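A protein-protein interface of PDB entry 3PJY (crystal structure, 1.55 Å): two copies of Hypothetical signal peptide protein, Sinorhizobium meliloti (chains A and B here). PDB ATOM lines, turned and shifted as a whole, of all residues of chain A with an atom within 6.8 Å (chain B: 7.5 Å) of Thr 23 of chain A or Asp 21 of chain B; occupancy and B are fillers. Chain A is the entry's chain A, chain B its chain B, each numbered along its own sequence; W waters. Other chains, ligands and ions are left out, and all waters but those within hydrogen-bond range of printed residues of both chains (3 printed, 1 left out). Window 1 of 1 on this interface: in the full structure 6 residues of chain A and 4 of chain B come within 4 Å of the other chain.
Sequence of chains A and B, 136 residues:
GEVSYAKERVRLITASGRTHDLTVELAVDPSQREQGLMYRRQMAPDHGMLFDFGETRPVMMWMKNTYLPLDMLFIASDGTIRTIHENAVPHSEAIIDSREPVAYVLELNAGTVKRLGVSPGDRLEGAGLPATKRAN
NH2 of Arg 9 of chain A lies within salt-bridge range of OD1 of Asp 21 of chain B.
The side-chain carboxylate of Asp 21 of chain B sits at hydrogen-bond distance from the side-chain hydroxyl of Thr 23 of chain A (2.9 Å).
NE of Arg 9 of chain B is in salt-bridge range of OD2 of Asp 46 of chain A (2.9 Å).
A ring nitrogen (NE2) of His 47 of chain A sits at hydrogen-bond distance from the guanidinium group (NH2) of Arg 9 of chain B (3.4 Å).
A ring nitrogen (NE2) of His 47 of chain A lies within hydrogen-bond range of the side-chain carboxylate (OD2) of Asp 21 of chain B, at 2.6 Å.
The side-chain hydroxyl (OG1) of Thr 23 of chain A is in hydrogen-bond range of the guanidinium group (NH2) of Arg 9 of chain A, at 2.9 Å.
O of Asp 46 of chain A lies within hydrogen-bond range of N of Thr 23 of chain A (3.0 Å).
O of Thr 23 of chain A lies within hydrogen-bond range of N of Gly 48 of chain A (3.2 Å).
The side-chain hydroxyl (OG1) of Thr 23 of chain B is in hydrogen-bond range of the guanidinium group (NH1) of Arg 9 of chain B (3.0 Å).
NH1 of Arg 11 of chain B is in hydrogen-bond range of OG1 of Thr 19 of chain B (3.0 Å).
O of Arg 11 of chain B lies within hydrogen-bond range of N of Glu 125 of chain B (2.8 Å).
Thr 19 of chain B touches Lys 7 of chain A (O to CD, 3.7 Å).
CG of Arg 9 of chain A touches NH1 of Arg 11 of chain B, at 3.0 Å.
Thr 23 of chain A touches Thr 19 of chain B.
Ala 44 of chain A touches Arg 9 of chain B.
Thr 23 of chain A touches just these residues of chain B: Thr 19 and Asp 21.
Asp 21 of chain B touches just these residues of chain A: Arg 9, Thr 23 and His 47.
Printed residues of chain B within 4 Å of Ala 44 of chain A: Arg 9 (3.6 Å).
Of the printed residues of chain B, Asp 46 of chain A touches Arg 9.
Printed residues of chain B within 4 Å of His 47 of chain A: Arg 9 and Asp 21.
Of the printed residues of chain A, Thr 19 of chain B touches Lys 7 and Thr 23.
Glu 8 of chain A touches none of the printed residues of chain B.
Pro 45 of chain B touches none of the printed residues of chain A.
The nearest residue of chain B that does not touch Thr 23 of chain A is Arg 11 of chain B (5.3 Å).
Of the 15 printed residues of chain A, 6 touch a printed residue of chain B.
Hydrophobic or aromatic side chains of chain A within 4 Å of the printed part of chain B: Ala 44 and His 47.
Arg 9 of chain A touches Asp 21 of chain B, but with the chains exchanged Asp 21 of chain A does not touch Arg 9 of chain B (7.6 Å).
Thr 23 of chain A touches Asp 21 of chain B, but with the chains exchanged Asp 21 of chain A does not touch Thr 23 of chain B (11.8 Å).
His 47 of chain A touches Arg 9 of chain B, but with the chains exchanged Arg 9 of chain A does not touch His 47 of chain B (14.5 Å).
His 47 of chain A touches Asp 21 of chain B, but with the chains exchanged Asp 21 of chain A does not touch His 47 of chain B (15.6 Å).
Of the 9 pairs that touch across the chains among the printed residues, none has its exchanged pair printed and touching as well.
Water W3 lies within hydrogen-bond range of the side-chain hydroxyl (OG1) of Thr 19 of chain B (2.6 Å), the side-chain carboxylate (OD1) of Asp 21 of chain B (2.6 Å) and the side-chain hydroxyl (OG1) of Thr 23 of chain A (2.6 Å).
Water W1 bridges N of Thr 19 of chain B and O of Lys 7 of chain A.
Water W2 lies within hydrogen-bond range of the side-chain carboxylate (OD1) of Asp 46 of chain A (3.0 Å) and the guanidinium group (NE) of Arg 9 of chain B (3.3 Å).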
ATOM      1  N   LYS A   7      11.298  -9.172  13.977  1.00  0.00           N
ATOM      2  CA  LYS A   7      11.077  -7.885  14.656  1.00  0.00           C
ATOM      3  C   LYS A   7       9.583  -7.546  14.599  1.00  0.00           C
ATOM      4  O   LYS A   7       9.004  -7.542  13.510  1.00  0.00           O
ATOM      5  CB  LYS A   7      11.970  -6.831  14.009  1.00  0.00           C
ATOM      6  CG  LYS A   7      11.925  -5.455  14.626  1.00  0.00           C
ATOM      7  CD  LYS A   7      12.745  -4.438  13.847  1.00  0.00           C
ATOM      8  CE  LYS A   7      14.222  -4.405  14.247  1.00  0.00           C
ATOM      9  NZ  LYS A   7      14.959  -3.282  13.555  1.00  0.00           N
ATOM     10  N   GLU A   8       8.966  -7.312  15.771  1.00  0.00           N
ATOM     11  CA  GLU A   8       7.499  -7.369  16.002  1.00  0.00           C
ATOM     12  C   GLU A   8       7.000  -6.122  16.740  1.00  0.00           C
ATOM     13  O   GLU A   8       7.715  -5.595  17.603  1.00  0.00           O
ATOM     14  CB  GLU A   8       7.158  -8.593  16.885  1.00  0.00           C
ATOM     15  CG  GLU A   8       5.664  -8.866  17.224  1.00  0.00           C
ATOM     16  CD  GLU A   8       5.461  -9.972  18.276  1.00  0.00           C
ATOM     17  OE1 GLU A   8       6.463 -10.425  18.887  1.00  0.00           O
ATOM     18  OE2 GLU A   8       4.302 -10.381  18.520  1.00  0.00           O
ATOM     19  N   ARG A   9       5.784  -5.660  16.414  1.00  0.00           N
ATOM     20  CA  ARG A   9       5.110  -4.671  17.261  1.00  0.00           C
ATOM     21  C   ARG A   9       4.363  -5.408  18.336  1.00  0.00           C
ATOM     22  O   ARG A   9       3.576  -6.335  18.070  1.00  0.00           O
ATOM     23  CB  ARG A   9       4.101  -3.863  16.446  1.00  0.00           C
ATOM     24  CG  ARG A   9       4.700  -2.744  15.691  1.00  0.00           C
ATOM     25  CD  ARG A   9       5.398  -1.689  16.555  1.00  0.00           C
ATOM     26  NE  ARG A   9       4.590  -0.521  16.891  1.00  0.00           N
ATOM     27  CZ  ARG A   9       5.068   0.532  17.552  1.00  0.00           C
ATOM     28  NH1 ARG A   9       4.269   1.570  17.822  1.00  0.00           N
ATOM     29  NH2 ARG A   9       6.342   0.555  17.957  1.00  0.00           N
ATOM     30  N   VAL A  10       4.588  -4.984  19.568  1.00  0.00           N
ATOM     31  CA  VAL A  10       3.900  -5.545  20.696  1.00  0.00           C
ATOM     32  C   VAL A  10       3.363  -4.367  21.497  1.00  0.00           C
ATOM     33  O   VAL A  10       3.670  -3.198  21.227  1.00  0.00           O
ATOM     34  CB  VAL A  10       4.781  -6.459  21.554  1.00  0.00           C
ATOM     35  CG1 VAL A  10       5.289  -7.643  20.753  1.00  0.00           C
ATOM     36  CG2 VAL A  10       5.969  -5.658  22.164  1.00  0.00           C
ATOM     37  N   ASP A  21       2.884   0.989  22.969  1.00  0.00           N
ATOM     38  CA  ASP A  21       3.409   0.204  21.875  1.00  0.00           C
ATOM     39  C   ASP A  21       4.932   0.201  21.852  1.00  0.00           C
ATOM     40  O   ASP A  21       5.605   1.211  22.156  1.00  0.00           O
ATOM     41  CB  ASP A  21       2.827   0.708  20.575  1.00  0.00           C
ATOM     42  CG  ASP A  21       1.302   0.418  20.480  1.00  0.00           C
ATOM     43  OD1 ASP A  21       0.775  -0.256  21.396  1.00  0.00           O
ATOM     44  OD2 ASP A  21       0.668   0.886  19.555  1.00  0.00           O
ATOM     45  N   LEU A  22       5.464  -0.954  21.493  1.00  0.00           N
ATOM     46  CA  LEU A  22       6.904  -1.193  21.395  1.00  0.00           C
ATOM     47  C   LEU A  22       7.219  -1.954  20.122  1.00  0.00           C
ATOM     48  O   LEU A  22       6.387  -2.666  19.576  1.00  0.00           O
ATOM     49  CB  LEU A  22       7.412  -2.038  22.569  1.00  0.00           C
ATOM     50  CG  LEU A  22       7.058  -1.588  23.975  1.00  0.00           C
ATOM     51  CD1 LEU A  22       7.271  -2.748  24.992  1.00  0.00           C
ATOM     52  CD2 LEU A  22       7.846  -0.357  24.370  1.00  0.00           C
ATOM     53  N   THR A  23       8.470  -1.849  19.680  1.00  0.00           N
ATOM     54  CA  THR A  23       8.975  -2.742  18.640  1.00  0.00           C
ATOM     55  C   THR A  23      10.082  -3.549  19.264  1.00  0.00           C
ATOM     56  O   THR A  23      11.020  -2.965  19.827  1.00  0.00           O
ATOM     57  CB  THR A  23       9.546  -1.956  17.431  1.00  0.00           C
ATOM     58  OG1 THR A  23       8.521  -1.110  16.889  1.00  0.00           O
ATOM     59  CG2 THR A  23      10.002  -2.919  16.320  1.00  0.00           C
ATOM     60  N   VAL A  24       9.959  -4.870  19.185  1.00  0.00           N
ATOM     61  CA  VAL A  24      10.933  -5.746  19.785  1.00  0.00           C
ATOM     62  C   VAL A  24      11.555  -6.696  18.796  1.00  0.00           C
ATOM     63  O   VAL A  24      10.902  -7.153  17.834  1.00  0.00           O
ATOM     64  CB  VAL A  24      10.334  -6.584  20.933  1.00  0.00           C
ATOM     65  CG1 VAL A  24       9.861  -5.623  22.072  1.00  0.00           C
ATOM     66  CG2 VAL A  24       9.169  -7.470  20.487  1.00  0.00           C
ATOM     67  N   GLU A  25      12.832  -6.996  19.020  1.00  0.00           N
ATOM     68  CA  GLU A  25      13.497  -8.094  18.347  1.00  0.00           C
ATOM     69  C   GLU A  25      13.271  -9.388  19.122  1.00  0.00           C
ATOM     70  O   GLU A  25      13.379  -9.384  20.350  1.00  0.00           O
ATOM     71  CB  GLU A  25      14.993  -7.802  18.245  1.00  0.00           C
ATOM     72  CG  GLU A  25      15.305  -6.728  17.174  1.00  0.00           C
ATOM     73  CD  GLU A  25      16.755  -6.240  17.233  1.00  0.00           C
ATOM     74  OE1 GLU A  25      17.312  -6.054  18.351  1.00  0.00           O
ATOM     75  OE2 GLU A  25      17.346  -6.047  16.156  1.00  0.00           O
ATOM     76  N   ALA A  44      16.289   2.750  21.424  1.00  0.00           N
ATOM     77  CA  ALA A  44      15.200   3.720  21.587  1.00  0.00           C
ATOM     78  C   ALA A  44      14.314   3.349  22.756  1.00  0.00           C
ATOM     79  O   ALA A  44      14.225   2.187  23.110  1.00  0.00           O
ATOM     80  CB  ALA A  44      14.374   3.853  20.303  1.00  0.00           C
ATOM     81  N   ASP A  46      11.207   3.051  23.077  1.00  0.00           N
ATOM     82  CA  ASP A  46      10.099   2.166  22.693  1.00  0.00           C
ATOM     83  C   ASP A  46      10.603   0.900  21.992  1.00  0.00           C
ATOM     84  O   ASP A  46       9.825   0.218  21.333  1.00  0.00           O
ATOM     85  CB  ASP A  46       9.063   2.890  21.849  1.00  0.00           C
ATOM     86  CG  ASP A  46       9.620   3.436  20.579  1.00  0.00           C
ATOM     87  OD1 ASP A  46      10.845   3.384  20.353  1.00  0.00           O
ATOM     88  OD2 ASP A  46       8.807   4.010  19.809  1.00  0.00           O
ATOM     89  N   HIS A  47      11.887   0.572  22.160  1.00  0.00           N
ATOM     90  CA  HIS A  47      12.444  -0.670  21.629  1.00  0.00           C
ATOM     91  C   HIS A  47      12.873  -1.598  22.752  1.00  0.00           C
ATOM     92  O   HIS A  47      13.181  -1.174  23.850  1.00  0.00           O
ATOM     93  CB  HIS A  47      13.652  -0.429  20.706  1.00  0.00           C
ATOM     94  CG  HIS A  47      13.278   0.226  19.418  1.00  0.00           C
ATOM     95  ND1 HIS A  47      14.208   0.646  18.490  1.00  0.00           N
ATOM     96  CD2 HIS A  47      12.062   0.519  18.903  1.00  0.00           C
ATOM     97  CE1 HIS A  47      13.562   1.186  17.455  1.00  0.00           C
ATOM     98  NE2 HIS A  47      12.260   1.105  17.672  1.00  0.00           N
ATOM     99  N   GLY A  48      12.893  -2.883  22.445  1.00  0.00           N
ATOM    100  CA  GLY A  48      13.412  -3.867  23.390  1.00  0.00           C
ATOM    101  C   GLY A  48      13.648  -5.188  22.721  1.00  0.00           C
ATOM    102  O   GLY A  48      13.632  -5.321  21.479  1.00  0.00           O
ATOM    103  N   MET A  49      13.923  -6.193  23.540  1.00  0.00           N
ATOM    104  CA  MET A  49      14.103  -7.550  23.018  1.00  0.00           C
ATOM    105  C   MET A  49      13.186  -8.458  23.798  1.00  0.00           C
ATOM    106  O   MET A  49      13.080  -8.352  25.046  1.00  0.00           O
ATOM    107  CB  MET A  49      15.560  -7.998  23.110  1.00  0.00           C
ATOM    108  CG  MET A  49      15.843  -9.397  22.653  1.00  0.00           C
ATOM    109  SD  MET A  49      17.704  -9.783  22.360  1.00  0.00           S
ATOM    110  CE  MET A  49      18.010  -8.835  20.682  1.00  0.00           C
ATOM    111  N   LEU A 108      13.798  -4.027  28.320  1.00  0.00           N
ATOM    112  CA  LEU A 108      13.580  -2.669  27.894  1.00  0.00           C
ATOM    113  C   LEU A 108      14.696  -1.819  28.483  1.00  0.00           C
ATOM    114  O   LEU A 108      15.378  -2.243  29.442  1.00  0.00           O
ATOM    115  CB  LEU A 108      12.227  -2.150  28.402  1.00  0.00           C
ATOM    116  CG  LEU A 108      11.007  -2.951  27.945  1.00  0.00           C
ATOM    117  CD1 LEU A 108       9.765  -2.518  28.692  1.00  0.00           C
ATOM    118  CD2 LEU A 108      10.870  -2.865  26.459  1.00  0.00           C
ATOM    119  N   ARG B   9       6.517   9.446  17.026  1.00  0.00           N
ATOM    120  CA  ARG B   9       6.985   8.174  16.526  1.00  0.00           C
ATOM    121  C   ARG B   9       6.032   7.709  15.436  1.00  0.00           C
ATOM    122  O   ARG B   9       4.802   7.728  15.593  1.00  0.00           O
ATOM    123  CB  ARG B   9       7.133   7.167  17.683  1.00  0.00           C
ATOM    124  CG  ARG B   9       8.227   7.549  18.653  1.00  0.00           C
ATOM    125  CD  ARG B   9       9.585   7.357  17.995  1.00  0.00           C
ATOM    126  NE  ARG B   9      10.165   5.993  18.134  1.00  0.00           N
ATOM    127  CZ  ARG B   9      11.318   5.664  17.568  1.00  0.00           C
ATOM    128  NH1 ARG B   9      11.943   6.564  16.802  1.00  0.00           N
ATOM    129  NH2 ARG B   9      11.864   4.464  17.771  1.00  0.00           N
ATOM    130  N   VAL B  10       6.618   7.354  14.302  1.00  0.00           N
ATOM    131  CA  VAL B  10       5.881   6.744  13.217  1.00  0.00           C
ATOM    132  C   VAL B  10       6.659   5.490  12.813  1.00  0.00           C
ATOM    133  O   VAL B  10       7.816   5.268  13.208  1.00  0.00           O
ATOM    134  CB  VAL B  10       5.690   7.690  12.035  1.00  0.00           C
ATOM    135  CG1 VAL B  10       4.900   8.903  12.490  1.00  0.00           C
ATOM    136  CG2 VAL B  10       7.033   8.096  11.414  1.00  0.00           C
ATOM    137  N   ARG B  11       6.033   4.689  11.981  1.00  0.00           N
ATOM    138  CA  ARG B  11       6.722   3.532  11.452  1.00  0.00           C
ATOM    139  C   ARG B  11       6.379   3.258  10.029  1.00  0.00           C
ATOM    140  O   ARG B  11       5.247   3.490   9.580  1.00  0.00           O
ATOM    141  CB  ARG B  11       6.471   2.315  12.271  1.00  0.00           C
ATOM    142  CG  ARG B  11       5.063   1.841  12.331  1.00  0.00           C
ATOM    143  CD  ARG B  11       4.873   0.921  13.568  1.00  0.00           C
ATOM    144  NE  ARG B  11       3.564   0.232  13.537  1.00  0.00           N
ATOM    145  CZ  ARG B  11       3.346  -1.051  13.189  1.00  0.00           C
ATOM    146  NH1 ARG B  11       4.349  -1.885  12.858  1.00  0.00           N
ATOM    147  NH2 ARG B  11       2.099  -1.535  13.197  1.00  0.00           N
ATOM    148  N   LEU B  12       7.397   2.830   9.316  1.00  0.00           N
ATOM    149  CA  LEU B  12       7.243   2.333   7.955  1.00  0.00           C
ATOM    150  C   LEU B  12       7.117   0.831   7.995  1.00  0.00           C
ATOM    151  O   LEU B  12       7.877   0.170   8.704  1.00  0.00           O
ATOM    152  CB  LEU B  12       8.442   2.749   7.094  1.00  0.00           C
ATOM    153  CG  LEU B  12       8.590   4.207   6.728  1.00  0.00           C
ATOM    154  CD1 LEU B  12       9.974   4.565   6.151  1.00  0.00           C
ATOM    155  CD2 LEU B  12       7.493   4.579   5.707  1.00  0.00           C
ATOM    156  N   THR B  19       9.150  -3.762   9.897  1.00  0.00           N
ATOM    157  CA  THR B  19       8.720  -2.511  10.494  1.00  0.00           C
ATOM    158  C   THR B  19       9.963  -1.757  10.902  1.00  0.00           C
ATOM    159  O   THR B  19      10.947  -2.344  11.339  1.00  0.00           O
ATOM    160  CB  THR B  19       7.764  -2.764  11.703  1.00  0.00           C
ATOM    161  OG1 THR B  19       7.212  -1.503  12.156  1.00  0.00           O
ATOM    162  CG2 THR B  19       8.444  -3.467  12.798  1.00  0.00           C
ATOM    163  N   HIS B  20       9.912  -0.442  10.725  1.00  0.00           N
ATOM    164  CA  HIS B  20      11.009   0.427  11.134  1.00  0.00           C
ATOM    165  C   HIS B  20      10.495   1.753  11.668  1.00  0.00           C
ATOM    166  O   HIS B  20       9.758   2.439  11.001  1.00  0.00           O
ATOM    167  CB  HIS B  20      11.962   0.698  10.004  1.00  0.00           C
ATOM    168  CG  HIS B  20      13.265   1.284  10.462  1.00  0.00           C
ATOM    169  ND1 HIS B  20      14.370   0.511  10.745  1.00  0.00           N
ATOM    170  CD2 HIS B  20      13.635   2.578  10.670  1.00  0.00           C
ATOM    171  CE1 HIS B  20      15.358   1.312  11.130  1.00  0.00           C
ATOM    172  NE2 HIS B  20      14.935   2.568  11.071  1.00  0.00           N
ATOM    173  N   ASP B  21      10.921   2.102  12.865  1.00  0.00           N
ATOM    174  CA  ASP B  21      10.489   3.313  13.503  1.00  0.00           C
ATOM    175  C   ASP B  21      11.333   4.524  13.151  1.00  0.00           C
ATOM    176  O   ASP B  21      12.574   4.427  12.975  1.00  0.00           O
ATOM    177  CB  ASP B  21      10.506   3.161  15.033  1.00  0.00           C
ATOM    178  CG  ASP B  21       9.574   2.085  15.528  1.00  0.00           C
ATOM    179  OD1 ASP B  21       8.436   1.935  15.036  1.00  0.00           O
ATOM    180  OD2 ASP B  21       9.951   1.391  16.469  1.00  0.00           O
ATOM    181  N   LEU B  22      10.645   5.653  13.074  1.00  0.00           N
ATOM    182  CA  LEU B  22      11.227   6.952  12.842  1.00  0.00           C
ATOM    183  C   LEU B  22      10.665   7.950  13.826  1.00  0.00           C
ATOM    184  O   LEU B  22       9.532   7.797  14.337  1.00  0.00           O
ATOM    185  CB  LEU B  22      10.949   7.476  11.409  1.00  0.00           C
ATOM    186  CG  LEU B  22      11.285   6.566  10.242  1.00  0.00           C
ATOM    187  CD1 LEU B  22      10.563   7.030   8.942  1.00  0.00           C
ATOM    188  CD2 LEU B  22      12.800   6.502  10.052  1.00  0.00           C
ATOM    189  N   THR B  23      11.415   9.021  14.052  1.00  0.00           N
ATOM    190  CA  THR B  23      10.913  10.173  14.808  1.00  0.00           C
ATOM    191  C   THR B  23      10.813  11.302  13.804  1.00  0.00           C
ATOM    192  O   THR B  23      11.772  11.595  13.097  1.00  0.00           O
ATOM    193  CB  THR B  23      11.881  10.596  15.874  1.00  0.00           C
ATOM    194  OG1 THR B  23      11.996   9.546  16.834  1.00  0.00           O
ATOM    195  CG2 THR B  23      11.335  11.826  16.584  1.00  0.00           C
ATOM    196  N   PRO B  45      19.792   9.563  11.086  1.00  0.00           N
ATOM    197  CA  PRO B  45      19.281   8.687  10.042  1.00  0.00           C
ATOM    198  C   PRO B  45      17.815   8.236  10.224  1.00  0.00           C
ATOM    199  O   PRO B  45      17.092   8.046   9.240  1.00  0.00           O
ATOM    200  CB  PRO B  45      20.169   7.450  10.135  1.00  0.00           C
ATOM    201  CG  PRO B  45      21.461   7.967  10.697  1.00  0.00           C
ATOM    202  CD  PRO B  45      21.074   9.062  11.659  1.00  0.00           C
ATOM    203  N   ASP B  46      17.381   8.068  11.468  1.00  0.00           N
ATOM    204  CA  ASP B  46      15.987   7.684  11.740  1.00  0.00           C
ATOM    205  C   ASP B  46      15.071   8.887  12.070  1.00  0.00           C
ATOM    206  O   ASP B  46      14.010   8.697  12.704  1.00  0.00           O
ATOM    207  CB  ASP B  46      15.912   6.603  12.821  1.00  0.00           C
ATOM    208  CG  ASP B  46      16.512   5.273  12.370  1.00  0.00           C
ATOM    209  OD1 ASP B  46      16.329   4.872  11.209  1.00  0.00           O
ATOM    210  OD2 ASP B  46      17.252   4.668  13.186  1.00  0.00           O
ATOM    211  N   HIS B  47      15.470  10.088  11.660  1.00  0.00           N
ATOM    212  CA  HIS B  47      14.666  11.283  11.843  1.00  0.00           C
ATOM    213  C   HIS B  47      14.278  11.875  10.491  1.00  0.00           C
ATOM    214  O   HIS B  47      15.065  11.878   9.546  1.00  0.00           O
ATOM    215  CB  HIS B  47      15.411  12.326  12.641  1.00  0.00           C
ATOM    216  CG  HIS B  47      15.450  12.056  14.113  1.00  0.00           C
ATOM    217  ND1 HIS B  47      14.767  12.840  15.025  1.00  0.00           N
ATOM    218  CD2 HIS B  47      16.121  11.128  14.839  1.00  0.00           C
ATOM    219  CE1 HIS B  47      15.009  12.389  16.249  1.00  0.00           C
ATOM    220  NE2 HIS B  47      15.825  11.358  16.163  1.00  0.00           N
ATOM    221  N   ARG B 115      18.069   2.028   2.420  1.00  0.00           N
ATOM    222  CA  ARG B 115      18.519   1.440   3.668  1.00  0.00           C
ATOM    223  C   ARG B 115      17.430   0.624   4.334  1.00  0.00           C
ATOM    224  O   ARG B 115      17.732  -0.455   4.889  1.00  0.00           O
ATOM    225  CB  ARG B 115      19.016   2.505   4.656  1.00  0.00           C
ATOM    226  CG  ARG B 115      19.380   1.964   6.073  1.00  0.00           C
ATOM    227  CD  ARG B 115      20.049   3.096   6.876  1.00  0.00           C
ATOM    228  NE  ARG B 115      19.147   4.189   7.319  1.00  0.00           N
ATOM    229  CZ  ARG B 115      18.420   4.170   8.431  1.00  0.00           C
ATOM    230  NH1 ARG B 115      18.374   3.101   9.225  1.00  0.00           N
ATOM    231  NH2 ARG B 115      17.751   5.257   8.783  1.00  0.00           N
ATOM    232  N   LEU B 116      16.177   1.060   4.208  1.00  0.00           N
ATOM    233  CA  LEU B 116      15.040   0.438   4.916  1.00  0.00           C
ATOM    234  C   LEU B 116      14.268  -0.572   4.058  1.00  0.00           C
ATOM    235  O   LEU B 116      13.357  -1.216   4.571  1.00  0.00           O
ATOM    236  CB  LEU B 116      14.133   1.512   5.489  1.00  0.00           C
ATOM    237  CG  LEU B 116      14.757   2.478   6.511  1.00  0.00           C
ATOM    238  CD1 LEU B 116      13.650   3.459   7.002  1.00  0.00           C
ATOM    239  CD2 LEU B 116      15.407   1.711   7.662  1.00  0.00           C
ATOM    240  N   GLU B 125       2.586   4.436   9.310  1.00  0.00           N
ATOM    241  CA  GLU B 125       1.600   4.308  10.386  1.00  0.00           C
ATOM    242  C   GLU B 125       2.051   5.159  11.544  1.00  0.00           C
ATOM    243  O   GLU B 125       3.254   5.328  11.818  1.00  0.00           O
ATOM    244  CB  GLU B 125       1.433   2.864  10.909  1.00  0.00           C
HETATM  245  O   HOH W   1      10.622  -5.929  11.167  1.00  0.00           O
HETATM  246  O   HOH W   2      11.050   6.218  21.322  1.00  0.00           O
HETATM  247  O   HOH W   3       8.088  -0.540  14.367  1.00  0.00           O
